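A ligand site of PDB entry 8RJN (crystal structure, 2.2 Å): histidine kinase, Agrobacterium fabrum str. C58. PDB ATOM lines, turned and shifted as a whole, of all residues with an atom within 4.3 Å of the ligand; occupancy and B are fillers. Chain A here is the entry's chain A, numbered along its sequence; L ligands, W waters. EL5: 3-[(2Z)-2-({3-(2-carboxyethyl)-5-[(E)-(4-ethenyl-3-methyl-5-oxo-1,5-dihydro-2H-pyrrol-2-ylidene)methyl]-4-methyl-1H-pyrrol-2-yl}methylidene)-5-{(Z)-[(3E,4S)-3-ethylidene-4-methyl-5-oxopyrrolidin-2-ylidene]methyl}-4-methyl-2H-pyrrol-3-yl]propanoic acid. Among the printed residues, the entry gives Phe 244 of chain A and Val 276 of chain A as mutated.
An oxygen (O2C) of the ligand lies within hydrogen-bond range of a ring nitrogen (NE2) of His 278 (2.8 Å). The backbone carbonyl oxygen of Asp 196 is in hydrogen-bond range of a nitrogen (NA) of the ligand (2.9 Å). The side-chain sulfur (SG) of Cys 13 is bonded to a carbon (CBA) of the ligand. The guanidinium group of Arg 211 lies within salt-bridge range of an oxygen (O1B) of the ligand, 2.8 Å away. OD of the ligand lies close to OH of Tyr 251, 3.1 Å away. ND of the ligand lies within hydrogen-bond range of OD2 of Asp 196 (3.3 Å). NH2 of Arg 242 is in salt-bridge range of O2B of the ligand (3.97 Å). OH of Tyr 165 is in hydrogen-bond range of O1C of the ligand.
OH of Tyr 251 is in hydrogen-bond range of OG of Ser 462 (2.6 Å). The side-chain hydroxyl (OG) of Ser 195 lies within hydrogen-bond range of the guanidinium group (NH2) of Arg 456 (3.3 Å). The side-chain hydroxyl (OG) of Ser 245 lies within hydrogen-bond range of the backbone NH (N) of Ile 247. NH1 of Arg 211 is in hydrogen-bond range of O of Arg 242 (2.8 Å). The side-chain carboxylate of Asp 196 lies within salt-bridge range of the guanidinium group of Arg 456 (2.7 Å). The side-chain amide nitrogen (NE2) of Gln 190 is in hydrogen-bond range of the backbone carbonyl oxygen (O) of Pro 459.
N of Asp 14 touches CBA of the ligand, 3.8 Å away. Phe 187 touches the ligand (CD2 to CBD, 3.5 Å). CB of Phe 192 touches ND of the ligand (3.8 Å). Ser 195 touches the ligand. Ile 197 touches the ligand (CG1 to NC, 3.9 Å). Pro 198 touches the ligand (CD to CHB, 3.3 Å). OH of Tyr 205 touches CAC of the ligand, at 3.1 Å. CB of Phe 244 touches O2B of the ligand, at 3.99 Å. CB of Ser 245 touches CMB of the ligand, at 3.8 Å. CG2 of Ile 247 touches C3A of the ligand, 3.7 Å away. ND1 of His 248 touches CHC of the ligand, at 3.3 Å. Met 255 touches the ligand. CG1 of Val 276 touches O1C of the ligand (3.2 Å). NH1 of Arg 456 touches OA of the ligand (3.8 Å). Leu 457 touches the ligand. CA of Pro 459 touches OD of the ligand (3.5 Å). Ser 462 touches the ligand. Hydrophobic or aromatic side chains within 4 Å of the ligand: Tyr 165, Phe 187, Phe 192, Ile 197, Pro 198, Phe 244, Ile 247, His 248, Tyr 251, Met 255, Val 276, His 278, Leu 457 and Pro 459. Within 4 Å of the ligand: Cys 13, Asp 14, Tyr 165, Phe 187, Phe 192, Ser 195, Asp 196, Ile 197, Pro 198, Tyr 205, Arg 211, Arg 242, Phe 244, Ser 245, Ile 247, His 248, Tyr 251, Met 255, Val 276, His 278, Arg 456, Leu 457, Pro 459 and Ser 462.
Water W1 lies within hydrogen-bond range of an oxygen (O2C) of the ligand, the side-chain hydroxyl of Ser 260 and a ring nitrogen (NE2) of His 248. Water W4 lies within hydrogen-bond range of O2B of the ligand and N of Ser 245. Water W2 bridges an oxygen (O1B) of the ligand (2.6 Å) and the side-chain hydroxyl (OH) of Tyr 205 (2.8 Å). Water W6 lies within hydrogen-bond range of an oxygen (O2B) of the ligand (2.7 Å) and the guanidinium group (NH2) of Arg 242 (2.7 Å). Water W3 bridges ND1 of His 248 (2.7 Å) and NC of the ligand (2.9 Å). Water W5 lies within hydrogen-bond range of NE2 of Gln 190 (2.7 Å) and OD of the ligand (3.0 Å).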
ATOM      1  N   CYS A  13     -27.317 -24.331  14.775  1.00  0.00           N
ATOM      2  CA  CYS A  13     -27.615 -23.158  15.646  1.00  0.00           C
ATOM      3  C   CYS A  13     -28.817 -22.371  15.111  1.00  0.00           C
ATOM      4  O   CYS A  13     -29.422 -21.601  15.898  1.00  0.00           O
ATOM      5  CB  CYS A  13     -26.398 -22.248  15.790  1.00  0.00           C
ATOM      6  SG  CYS A  13     -26.008 -21.316  14.279  1.00  0.00           S
ATOM      7  N   ASP A  14     -29.164 -22.562  13.834  1.00  0.00           N
ATOM      8  CA  ASP A  14     -30.382 -21.994  13.184  1.00  0.00           C
ATOM      9  C   ASP A  14     -31.647 -22.614  13.788  1.00  0.00           C
ATOM     10  O   ASP A  14     -32.712 -21.981  13.685  1.00  0.00           O
ATOM     11  CB  ASP A  14     -30.347 -22.191  11.667  1.00  0.00           C
ATOM     12  CG  ASP A  14     -30.327 -23.640  11.227  1.00  0.00           C
ATOM     13  OD1 ASP A  14     -29.493 -24.411  11.754  1.00  0.00           O
ATOM     14  OD2 ASP A  14     -31.145 -24.000  10.353  1.00  0.00           O
ATOM     15  N   ILE A  18     -33.481 -22.076  21.944  1.00  0.00           N
ATOM     16  CA  ILE A  18     -32.928 -21.046  22.878  1.00  0.00           C
ATOM     17  C   ILE A  18     -33.958 -20.687  23.962  1.00  0.00           C
ATOM     18  O   ILE A  18     -33.550 -20.048  24.951  1.00  0.00           O
ATOM     19  CB  ILE A  18     -32.464 -19.790  22.108  1.00  0.00           C
ATOM     20  CG1 ILE A  18     -33.603 -19.136  21.313  1.00  0.00           C
ATOM     21  CG2 ILE A  18     -31.282 -20.132  21.217  1.00  0.00           C
ATOM     22  CD1 ILE A  18     -33.315 -17.715  20.895  1.00  0.00           C
ATOM     23  N   TYR A 165     -30.448  -1.406  14.590  1.00  0.00           N
ATOM     24  CA  TYR A 165     -30.595  -2.273  13.389  1.00  0.00           C
ATOM     25  C   TYR A 165     -32.001  -2.091  12.833  1.00  0.00           C
ATOM     26  O   TYR A 165     -32.969  -2.108  13.623  1.00  0.00           O
ATOM     27  CB  TYR A 165     -30.361  -3.744  13.726  1.00  0.00           C
ATOM     28  CG  TYR A 165     -29.166  -4.034  14.588  1.00  0.00           C
ATOM     29  CD1 TYR A 165     -27.908  -3.574  14.252  1.00  0.00           C
ATOM     30  CD2 TYR A 165     -29.284  -4.816  15.727  1.00  0.00           C
ATOM     31  CE1 TYR A 165     -26.799  -3.846  15.037  1.00  0.00           C
ATOM     32  CE2 TYR A 165     -28.183  -5.106  16.525  1.00  0.00           C
ATOM     33  CZ  TYR A 165     -26.936  -4.617  16.179  1.00  0.00           C
ATOM     34  OH  TYR A 165     -25.859  -4.917  16.963  1.00  0.00           O
ATOM     35  N   PHE A 187     -19.661   0.409  13.179  1.00  0.00           N
ATOM     36  CA  PHE A 187     -20.440  -0.579  12.380  1.00  0.00           C
ATOM     37  C   PHE A 187     -21.496   0.126  11.524  1.00  0.00           C
ATOM     38  O   PHE A 187     -22.330  -0.563  10.930  1.00  0.00           O
ATOM     39  CB  PHE A 187     -21.106  -1.604  13.298  1.00  0.00           C
ATOM     40  CG  PHE A 187     -20.163  -2.427  14.133  1.00  0.00           C
ATOM     41  CD1 PHE A 187     -19.105  -3.102  13.545  1.00  0.00           C
ATOM     42  CD2 PHE A 187     -20.349  -2.556  15.498  1.00  0.00           C
ATOM     43  CE1 PHE A 187     -18.243  -3.866  14.311  1.00  0.00           C
ATOM     44  CE2 PHE A 187     -19.488  -3.320  16.265  1.00  0.00           C
ATOM     45  CZ  PHE A 187     -18.429  -3.975  15.675  1.00  0.00           C
ATOM     46  N   GLN A 190     -23.073  -0.876   7.942  1.00  0.00           N
ATOM     47  CA  GLN A 190     -22.747  -2.316   7.809  1.00  0.00           C
ATOM     48  C   GLN A 190     -24.038  -3.126   7.878  1.00  0.00           C
ATOM     49  O   GLN A 190     -24.920  -2.755   8.676  1.00  0.00           O
ATOM     50  CB  GLN A 190     -21.786  -2.738   8.920  1.00  0.00           C
ATOM     51  CG  GLN A 190     -21.051  -4.036   8.643  1.00  0.00           C
ATOM     52  CD  GLN A 190     -20.012  -4.335   9.700  1.00  0.00           C
ATOM     53  OE1 GLN A 190     -19.172  -3.505  10.028  1.00  0.00           O
ATOM     54  NE2 GLN A 190     -20.067  -5.535  10.251  1.00  0.00           N
ATOM     55  N   PHE A 192     -25.749  -7.222   8.322  1.00  0.00           N
ATOM     56  CA  PHE A 192     -25.558  -8.644   8.736  1.00  0.00           C
ATOM     57  C   PHE A 192     -26.648  -9.498   8.082  1.00  0.00           C
ATOM     58  O   PHE A 192     -27.764  -9.041   7.879  1.00  0.00           O
ATOM     59  CB  PHE A 192     -25.520  -8.782  10.260  1.00  0.00           C
ATOM     60  CG  PHE A 192     -26.714  -8.288  11.041  1.00  0.00           C
ATOM     61  CD1 PHE A 192     -27.879  -9.043  11.112  1.00  0.00           C
ATOM     62  CD2 PHE A 192     -26.654  -7.102  11.758  1.00  0.00           C
ATOM     63  CE1 PHE A 192     -28.963  -8.597  11.844  1.00  0.00           C
ATOM     64  CE2 PHE A 192     -27.739  -6.666  12.490  1.00  0.00           C
ATOM     65  CZ  PHE A 192     -28.895  -7.413  12.549  1.00  0.00           C
ATOM     66  N   SER A 195     -29.420 -14.963   8.893  1.00  0.00           N
ATOM     67  CA  SER A 195     -28.981 -16.169   9.672  1.00  0.00           C
ATOM     68  C   SER A 195     -28.280 -15.771  10.976  1.00  0.00           C
ATOM     69  O   SER A 195     -28.251 -16.616  11.895  1.00  0.00           O
ATOM     70  CB  SER A 195     -28.099 -17.056   8.826  1.00  0.00           C
ATOM     71  OG  SER A 195     -26.937 -16.377   8.403  1.00  0.00           O
ATOM     72  N   ASP A 196     -27.736 -14.553  11.081  1.00  0.00           N
ATOM     73  CA  ASP A 196     -27.064 -14.048  12.313  1.00  0.00           C
ATOM     74  C   ASP A 196     -28.084 -13.866  13.447  1.00  0.00           C
ATOM     75  O   ASP A 196     -27.634 -13.730  14.595  1.00  0.00           O
ATOM     76  CB  ASP A 196     -26.300 -12.747  12.062  1.00  0.00           C
ATOM     77  CG  ASP A 196     -24.918 -12.944  11.468  1.00  0.00           C
ATOM     78  OD1 ASP A 196     -24.706 -13.969  10.788  1.00  0.00           O
ATOM     79  OD2 ASP A 196     -24.057 -12.073  11.686  1.00  0.00           O
ATOM     80  N   ILE A 197     -29.377 -13.821  13.144  1.00  0.00           N
ATOM     81  CA  ILE A 197     -30.473 -13.835  14.163  1.00  0.00           C
ATOM     82  C   ILE A 197     -31.509 -14.874  13.736  1.00  0.00           C
ATOM     83  O   ILE A 197     -32.386 -14.584  12.933  1.00  0.00           O
ATOM     84  CB  ILE A 197     -31.093 -12.436  14.370  1.00  0.00           C
ATOM     85  CG1 ILE A 197     -30.043 -11.367  14.659  1.00  0.00           C
ATOM     86  CG2 ILE A 197     -32.158 -12.486  15.457  1.00  0.00           C
ATOM     87  CD1 ILE A 197     -30.590  -9.963  14.717  1.00  0.00           C
ATOM     88  N   PRO A 198     -31.418 -16.124  14.261  1.00  0.00           N
ATOM     89  CA  PRO A 198     -32.367 -17.181  13.920  1.00  0.00           C
ATOM     90  C   PRO A 198     -33.834 -16.833  14.193  1.00  0.00           C
ATOM     91  O   PRO A 198     -34.096 -15.930  14.963  1.00  0.00           O
ATOM     92  CB  PRO A 198     -31.944 -18.367  14.813  1.00  0.00           C
ATOM     93  CG  PRO A 198     -30.494 -18.096  15.146  1.00  0.00           C
ATOM     94  CD  PRO A 198     -30.382 -16.582  15.197  1.00  0.00           C
ATOM     95  N   ALA A 201     -35.084 -16.695  17.790  1.00  0.00           N
ATOM     96  CA  ALA A 201     -34.566 -15.466  18.432  1.00  0.00           C
ATOM     97  C   ALA A 201     -35.454 -14.268  18.072  1.00  0.00           C
ATOM     98  O   ALA A 201     -35.787 -13.481  18.987  1.00  0.00           O
ATOM     99  CB  ALA A 201     -33.131 -15.230  18.024  1.00  0.00           C
ATOM    100  N   TYR A 205     -37.650 -11.816  20.520  1.00  0.00           N
ATOM    101  CA  TYR A 205     -37.493 -10.336  20.400  1.00  0.00           C
ATOM    102  C   TYR A 205     -38.879  -9.695  20.219  1.00  0.00           C
ATOM    103  O   TYR A 205     -39.089  -8.593  20.730  1.00  0.00           O
ATOM    104  CB  TYR A 205     -36.555  -9.964  19.246  1.00  0.00           C
ATOM    105  CG  TYR A 205     -35.084 -10.150  19.513  1.00  0.00           C
ATOM    106  CD1 TYR A 205     -34.497  -9.716  20.694  1.00  0.00           C
ATOM    107  CD2 TYR A 205     -34.255 -10.731  18.566  1.00  0.00           C
ATOM    108  CE1 TYR A 205     -33.140  -9.869  20.941  1.00  0.00           C
ATOM    109  CE2 TYR A 205     -32.892 -10.896  18.792  1.00  0.00           C
ATOM    110  CZ  TYR A 205     -32.333 -10.460  19.989  1.00  0.00           C
ATOM    111  OH  TYR A 205     -30.999 -10.623  20.221  1.00  0.00           O
ATOM    112  N   ARG A 211     -34.231  -7.530  26.272  1.00  0.00           N
ATOM    113  CA  ARG A 211     -33.375  -8.746  26.374  1.00  0.00           C
ATOM    114  C   ARG A 211     -32.055  -8.324  27.030  1.00  0.00           C
ATOM    115  O   ARG A 211     -31.349  -7.498  26.423  1.00  0.00           O
ATOM    116  CB  ARG A 211     -33.197  -9.380  24.989  1.00  0.00           C
ATOM    117  CG  ARG A 211     -32.125 -10.469  24.906  1.00  0.00           C
ATOM    118  CD  ARG A 211     -32.237 -11.473  26.039  1.00  0.00           C
ATOM    119  NE  ARG A 211     -31.528 -12.710  25.763  1.00  0.00           N
ATOM    120  CZ  ARG A 211     -31.384 -13.694  26.637  1.00  0.00           C
ATOM    121  NH1 ARG A 211     -31.881 -13.590  27.856  1.00  0.00           N
ATOM    122  NH2 ARG A 211     -30.722 -14.795  26.290  1.00  0.00           N
ATOM    123  N   ILE A 213     -28.271  -9.279  28.741  1.00  0.00           N
ATOM    124  CA  ILE A 213     -27.094 -10.168  28.971  1.00  0.00           C
ATOM    125  C   ILE A 213     -26.137  -9.427  29.915  1.00  0.00           C
ATOM    126  O   ILE A 213     -25.449  -8.510  29.449  1.00  0.00           O
ATOM    127  CB  ILE A 213     -26.432 -10.599  27.649  1.00  0.00           C
ATOM    128  CG1 ILE A 213     -27.411 -11.356  26.753  1.00  0.00           C
ATOM    129  CG2 ILE A 213     -25.171 -11.409  27.919  1.00  0.00           C
ATOM    130  CD1 ILE A 213     -26.831 -11.822  25.439  1.00  0.00           C
ATOM    131  N   ARG A 242     -33.366 -15.820  31.606  1.00  0.00           N
ATOM    132  CA  ARG A 242     -33.076 -16.882  30.606  1.00  0.00           C
ATOM    133  C   ARG A 242     -31.640 -16.735  30.081  1.00  0.00           C
ATOM    134  O   ARG A 242     -31.261 -15.617  29.695  1.00  0.00           O
ATOM    135  CB  ARG A 242     -34.051 -16.816  29.429  1.00  0.00           C
ATOM    136  CG  ARG A 242     -33.713 -17.762  28.278  1.00  0.00           C
ATOM    137  CD  ARG A 242     -34.785 -17.794  27.209  1.00  0.00           C
ATOM    138  NE  ARG A 242     -35.063 -16.456  26.685  1.00  0.00           N
ATOM    139  CZ  ARG A 242     -34.367 -15.846  25.737  1.00  0.00           C
ATOM    140  NH1 ARG A 242     -34.708 -14.626  25.347  1.00  0.00           N
ATOM    141  NH2 ARG A 242     -33.318 -16.428  25.175  1.00  0.00           N
ATOM    142  N   PHE A 244     -28.277 -17.300  27.537  1.00  0.00           N
ATOM    143  CA  PHE A 244     -28.061 -16.967  26.101  1.00  0.00           C
ATOM    144  C   PHE A 244     -27.317 -18.117  25.414  1.00  0.00           C
ATOM    145  O   PHE A 244     -26.596 -18.871  26.085  1.00  0.00           O
ATOM    146  CB  PHE A 244     -27.300 -15.635  25.982  1.00  0.00           C
ATOM    147  CG  PHE A 244     -26.143 -15.485  26.934  1.00  0.00           C
ATOM    148  CD1 PHE A 244     -26.327 -14.968  28.215  1.00  0.00           C
ATOM    149  CD2 PHE A 244     -24.850 -15.862  26.565  1.00  0.00           C
ATOM    150  CE1 PHE A 244     -25.267 -14.849  29.097  1.00  0.00           C
ATOM    151  CE2 PHE A 244     -23.789 -15.733  27.446  1.00  0.00           C
ATOM    152  CZ  PHE A 244     -23.998 -15.227  28.712  1.00  0.00           C
ATOM    153  N   SER A 245     -27.515 -18.248  24.093  1.00  0.00           N
ATOM    154  CA  SER A 245     -26.869 -19.275  23.233  1.00  0.00           C
ATOM    155  C   SER A 245     -25.350 -19.155  23.337  1.00  0.00           C
ATOM    156  O   SER A 245     -24.815 -18.046  23.329  1.00  0.00           O
ATOM    157  CB  SER A 245     -27.328 -19.152  21.804  1.00  0.00           C
ATOM    158  OG  SER A 245     -26.419 -19.821  20.929  1.00  0.00           O
ATOM    159  N   ILE A 247     -23.314 -19.793  21.025  1.00  0.00           N
ATOM    160  CA  ILE A 247     -22.934 -19.259  19.686  1.00  0.00           C
ATOM    161  C   ILE A 247     -22.823 -17.741  19.788  1.00  0.00           C
ATOM    162  O   ILE A 247     -21.807 -17.179  19.331  1.00  0.00           O
ATOM    163  CB  ILE A 247     -23.941 -19.687  18.599  1.00  0.00           C
ATOM    164  CG1 ILE A 247     -24.057 -21.217  18.479  1.00  0.00           C
ATOM    165  CG2 ILE A 247     -23.606 -19.051  17.263  1.00  0.00           C
ATOM    166  CD1 ILE A 247     -22.788 -21.910  18.033  1.00  0.00           C
ATOM    167  N   HIS A 248     -23.841 -17.088  20.380  1.00  0.00           N
ATOM    168  CA  HIS A 248     -23.889 -15.616  20.568  1.00  0.00           C
ATOM    169  C   HIS A 248     -22.843 -15.194  21.596  1.00  0.00           C
ATOM    170  O   HIS A 248     -22.172 -14.167  21.372  1.00  0.00           O
ATOM    171  CB  HIS A 248     -25.295 -15.142  20.953  1.00  0.00           C
ATOM    172  CG  HIS A 248     -25.401 -13.652  20.947  1.00  0.00           C
ATOM    173  ND1 HIS A 248     -25.106 -12.896  19.835  1.00  0.00           N
ATOM    174  CD2 HIS A 248     -25.748 -12.780  21.920  1.00  0.00           C
ATOM    175  CE1 HIS A 248     -25.259 -11.623  20.119  1.00  0.00           C
ATOM    176  NE2 HIS A 248     -25.655 -11.519  21.389  1.00  0.00           N
ATOM    177  N   TYR A 251     -19.658 -14.933  19.912  1.00  0.00           N
ATOM    178  CA  TYR A 251     -19.754 -13.752  19.015  1.00  0.00           C
ATOM    179  C   TYR A 251     -19.390 -12.484  19.798  1.00  0.00           C
ATOM    180  O   TYR A 251     -18.516 -11.715  19.335  1.00  0.00           O
ATOM    181  CB  TYR A 251     -21.139 -13.627  18.377  1.00  0.00           C
ATOM    182  CG  TYR A 251     -21.122 -12.904  17.058  1.00  0.00           C
ATOM    183  CD1 TYR A 251     -20.783 -11.561  16.971  1.00  0.00           C
ATOM    184  CD2 TYR A 251     -21.407 -13.563  15.871  1.00  0.00           C
ATOM    185  CE1 TYR A 251     -20.747 -10.891  15.764  1.00  0.00           C
ATOM    186  CE2 TYR A 251     -21.376 -12.904  14.645  1.00  0.00           C
ATOM    187  CZ  TYR A 251     -21.039 -11.568  14.600  1.00  0.00           C
ATOM    188  OH  TYR A 251     -21.001 -10.907  13.404  1.00  0.00           O
ATOM    189  N   LEU A 252     -20.036 -12.267  20.957  1.00  0.00           N
ATOM    190  CA  LEU A 252     -19.823 -11.077  21.826  1.00  0.00           C
ATOM    191  C   LEU A 252     -18.381 -11.082  22.353  1.00  0.00           C
ATOM    192  O   LEU A 252     -17.738 -10.008  22.336  1.00  0.00           O
ATOM    193  CB  LEU A 252     -20.830 -11.084  22.981  1.00  0.00           C
ATOM    194  CG  LEU A 252     -22.293 -10.887  22.599  1.00  0.00           C
ATOM    195  CD1 LEU A 252     -23.166 -10.823  23.845  1.00  0.00           C
ATOM    196  CD2 LEU A 252     -22.486  -9.626  21.757  1.00  0.00           C
ATOM    197  N   MET A 255     -15.967  -9.924  19.856  1.00  0.00           N
ATOM    198  CA  MET A 255     -16.144  -8.470  19.601  1.00  0.00           C
ATOM    199  C   MET A 255     -15.579  -7.635  20.760  1.00  0.00           C
ATOM    200  O   MET A 255     -15.429  -6.410  20.577  1.00  0.00           O
ATOM    201  CB  MET A 255     -17.616  -8.105  19.435  1.00  0.00           C
ATOM    202  CG  MET A 255     -18.219  -8.509  18.111  1.00  0.00           C
ATOM    203  SD  MET A 255     -19.983  -8.141  18.065  1.00  0.00           S
ATOM    204  CE  MET A 255     -19.955  -6.351  18.125  1.00  0.00           C
ATOM    205  N   SER A 260     -24.882  -6.805  27.105  1.00  0.00           N
ATOM    206  CA  SER A 260     -25.798  -6.249  26.077  1.00  0.00           C
ATOM    207  C   SER A 260     -27.186  -6.021  26.680  1.00  0.00           C
ATOM    208  O   SER A 260     -27.561  -6.735  27.631  1.00  0.00           O
ATOM    209  CB  SER A 260     -25.868  -7.122  24.851  1.00  0.00           C
ATOM    210  OG  SER A 260     -26.659  -8.274  25.077  1.00  0.00           O
ATOM    211  N   VAL A 276     -29.923  -1.680  20.310  1.00  0.00           N
ATOM    212  CA  VAL A 276     -29.003  -2.622  21.014  1.00  0.00           C
ATOM    213  C   VAL A 276     -27.910  -1.817  21.701  1.00  0.00           C
ATOM    214  O   VAL A 276     -27.238  -1.004  21.031  1.00  0.00           O
ATOM    215  CB  VAL A 276     -28.430  -3.675  20.048  1.00  0.00           C
ATOM    216  CG1 VAL A 276     -27.332  -4.509  20.689  1.00  0.00           C
ATOM    217  CG2 VAL A 276     -29.534  -4.570  19.493  1.00  0.00           C
ATOM    218  N   HIS A 278     -24.371  -2.256  23.714  1.00  0.00           N
ATOM    219  CA  HIS A 278     -23.187  -3.109  24.022  1.00  0.00           C
ATOM    220  C   HIS A 278     -22.307  -2.399  25.054  1.00  0.00           C
ATOM    221  O   HIS A 278     -22.106  -1.173  24.922  1.00  0.00           O
ATOM    222  CB  HIS A 278     -22.398  -3.452  22.750  1.00  0.00           C
ATOM    223  CG  HIS A 278     -23.083  -4.442  21.861  1.00  0.00           C
ATOM    224  ND1 HIS A 278     -22.639  -4.700  20.571  1.00  0.00           N
ATOM    225  CD2 HIS A 278     -24.165  -5.222  22.049  1.00  0.00           C
ATOM    226  CE1 HIS A 278     -23.417  -5.600  20.011  1.00  0.00           C
ATOM    227  NE2 HIS A 278     -24.354  -5.933  20.898  1.00  0.00           N
ATOM    228  N   ARG A 456     -16.455 -17.210  11.616  1.00  0.00           N
ATOM    229  CA  ARG A 456     -17.874 -17.004  11.245  1.00  0.00           C
ATOM    230  C   ARG A 456     -18.539 -16.035  12.235  1.00  0.00           C
ATOM    231  O   ARG A 456     -19.404 -15.256  11.806  1.00  0.00           O
ATOM    232  CB  ARG A 456     -18.624 -18.347  11.219  1.00  0.00           C
ATOM    233  CG  ARG A 456     -20.124 -18.227  10.983  1.00  0.00           C
ATOM    234  CD  ARG A 456     -20.471 -17.526   9.688  1.00  0.00           C
ATOM    235  NE  ARG A 456     -21.916 -17.364   9.509  1.00  0.00           N
ATOM    236  CZ  ARG A 456     -22.641 -16.352   9.977  1.00  0.00           C
ATOM    237  NH1 ARG A 456     -22.076 -15.371  10.677  1.00  0.00           N
ATOM    238  NH2 ARG A 456     -23.941 -16.321   9.747  1.00  0.00           N
ATOM    239  N   LEU A 457     -18.137 -16.088  13.507  1.00  0.00           N
ATOM    240  CA  LEU A 457     -18.739 -15.285  14.607  1.00  0.00           C
ATOM    241  C   LEU A 457     -17.963 -13.972  14.772  1.00  0.00           C
ATOM    242  O   LEU A 457     -17.595 -13.642  15.913  1.00  0.00           O
ATOM    243  CB  LEU A 457     -18.730 -16.132  15.889  1.00  0.00           C
ATOM    244  CG  LEU A 457     -19.342 -17.531  15.748  1.00  0.00           C
ATOM    245  CD1 LEU A 457     -19.343 -18.242  17.093  1.00  0.00           C
ATOM    246  CD2 LEU A 457     -20.748 -17.470  15.179  1.00  0.00           C
ATOM    247  N   PRO A 459     -18.045  -9.697  13.115  1.00  0.00           N
ATOM    248  CA  PRO A 459     -18.662  -8.713  12.223  1.00  0.00           C
ATOM    249  C   PRO A 459     -18.087  -8.716  10.798  1.00  0.00           C
ATOM    250  O   PRO A 459     -18.857  -8.571   9.861  1.00  0.00           O
ATOM    251  CB  PRO A 459     -18.335  -7.381  12.907  1.00  0.00           C
ATOM    252  CG  PRO A 459     -18.268  -7.734  14.379  1.00  0.00           C
ATOM    253  CD  PRO A 459     -17.681  -9.123  14.414  1.00  0.00           C
ATOM    254  N   SER A 462     -19.505 -11.798   9.010  1.00  0.00           N
ATOM    255  CA  SER A 462     -20.968 -11.499   8.907  1.00  0.00           C
ATOM    256  C   SER A 462     -21.216 -10.606   7.692  1.00  0.00           C
ATOM    257  O   SER A 462     -22.075 -10.951   6.866  1.00  0.00           O
ATOM    258  CB  SER A 462     -21.505 -10.877  10.181  1.00  0.00           C
ATOM    259  OG  SER A 462     -21.791 -11.874  11.154  1.00  0.00           O
HETATM  260  C1A EL5 L   1     -24.768 -15.950  14.429  1.00  0.00           C
HETATM  261  C1B EL5 L   1     -27.892 -15.786  17.523  1.00  0.00           C
HETATM  262  O1B EL5 L   1     -30.146 -12.609  23.279  1.00  0.00           O
HETATM  263  C1C EL5 L   1     -27.530 -11.473  17.685  1.00  0.00           C
HETATM  264  O1C EL5 L   1     -26.924  -7.191  18.924  1.00  0.00           O
HETATM  265  C1D EL5 L   1     -24.411  -9.416  14.761  1.00  0.00           C
HETATM  266  C2A EL5 L   1     -25.104 -17.238  14.050  1.00  0.00           C
HETATM  267  C2B EL5 L   1     -28.737 -15.926  18.613  1.00  0.00           C
HETATM  268  O2B EL5 L   1     -30.184 -14.821  23.341  1.00  0.00           O
HETATM  269  C2C EL5 L   1     -27.796 -10.110  17.628  1.00  0.00           C
HETATM  270  O2C EL5 L   1     -26.136  -8.102  20.758  1.00  0.00           O
HETATM  271  C2D EL5 L   1     -23.836  -8.437  15.561  1.00  0.00           C
HETATM  272  C3A EL5 L   1     -26.101 -17.775  14.850  1.00  0.00           C
HETATM  273  C3B EL5 L   1     -28.932 -14.662  19.152  1.00  0.00           C
HETATM  274  C3C EL5 L   1     -27.088  -9.590  16.561  1.00  0.00           C
HETATM  275  C3D EL5 L   1     -22.863  -7.785  14.810  1.00  0.00           C
HETATM  276  C4A EL5 L   1     -26.448 -16.740  15.721  1.00  0.00           C
HETATM  277  C4B EL5 L   1     -28.233 -13.781  18.338  1.00  0.00           C
HETATM  278  C4C EL5 L   1     -26.335 -10.602  15.975  1.00  0.00           C
HETATM  279  C4D EL5 L   1     -22.821  -8.374  13.552  1.00  0.00           C
HETATM  280  CAA EL5 L   1     -26.725 -19.032  14.712  1.00  0.00           C
HETATM  281  CAB EL5 L   1     -29.744 -14.293  20.355  1.00  0.00           C
HETATM  282  CAC EL5 L   1     -28.724  -9.337  18.531  1.00  0.00           C
HETATM  283  CAD EL5 L   1     -22.111  -6.663  15.227  1.00  0.00           C
HETATM  284  CBA EL5 L   1     -26.518 -19.881  13.694  1.00  0.00           C
HETATM  285  CBB EL5 L   1     -28.972 -13.804  21.577  1.00  0.00           C
HETATM  286  CBC EL5 L   1     -28.157  -8.979  19.895  1.00  0.00           C
HETATM  287  CBD EL5 L   1     -21.630  -5.688  14.473  1.00  0.00           C
HETATM  288  CGB EL5 L   1     -29.833 -13.741  22.830  1.00  0.00           C
HETATM  289  CGC EL5 L   1     -26.985  -8.021  19.851  1.00  0.00           C
HETATM  290  CHB EL5 L   1     -27.471 -16.794  16.657  1.00  0.00           C
HETATM  291  CHC EL5 L   1     -28.113 -12.407  18.530  1.00  0.00           C
HETATM  292  CHD EL5 L   1     -25.463 -10.329  14.932  1.00  0.00           C
HETATM  293  CMA EL5 L   1     -24.047 -18.123  13.466  1.00  0.00           C
HETATM  294  CMB EL5 L   1     -29.298 -17.205  19.159  1.00  0.00           C
HETATM  295  CMC EL5 L   1     -27.093  -8.156  16.150  1.00  0.00           C
HETATM  296  CMD EL5 L   1     -24.134  -8.075  16.988  1.00  0.00           C
HETATM  297  NA  EL5 L   1     -25.625 -15.641  15.471  1.00  0.00           N
HETATM  298  OA  EL5 L   1     -23.903 -15.239  13.992  1.00  0.00           O
HETATM  299  NB  EL5 L   1     -27.630 -14.458  17.311  1.00  0.00           N
HETATM  300  NC  EL5 L   1     -26.707 -11.772  16.619  1.00  0.00           N
HETATM  301  ND  EL5 L   1     -23.763  -9.377  13.533  1.00  0.00           N
HETATM  302  OD  EL5 L   1     -22.104  -8.097  12.602  1.00  0.00           O
HETATM  303  O   HOH W   1     -26.934  -9.329  22.769  1.00  0.00           O
HETATM  304  O   HOH W   2     -29.490 -10.164  22.544  1.00  0.00           O
HETATM  305  O   HOH W   3     -24.486 -13.525  17.329  1.00  0.00           O
HETATM  306  O   HOH W   4     -29.862 -17.383  22.966  1.00  0.00           O
HETATM  307  O   HOH W   5     -22.166  -7.205   9.754  1.00  0.00           O
HETATM  308  O   HOH W   6     -32.865 -14.816  23.004  1.00  0.00           O
HETATM  309  O   HOH W   7     -29.152 -19.100  11.966  1.00  0.00           O
HETATM  310  O   HOH W   8     -27.417 -20.507  10.584  1.00  0.00           O
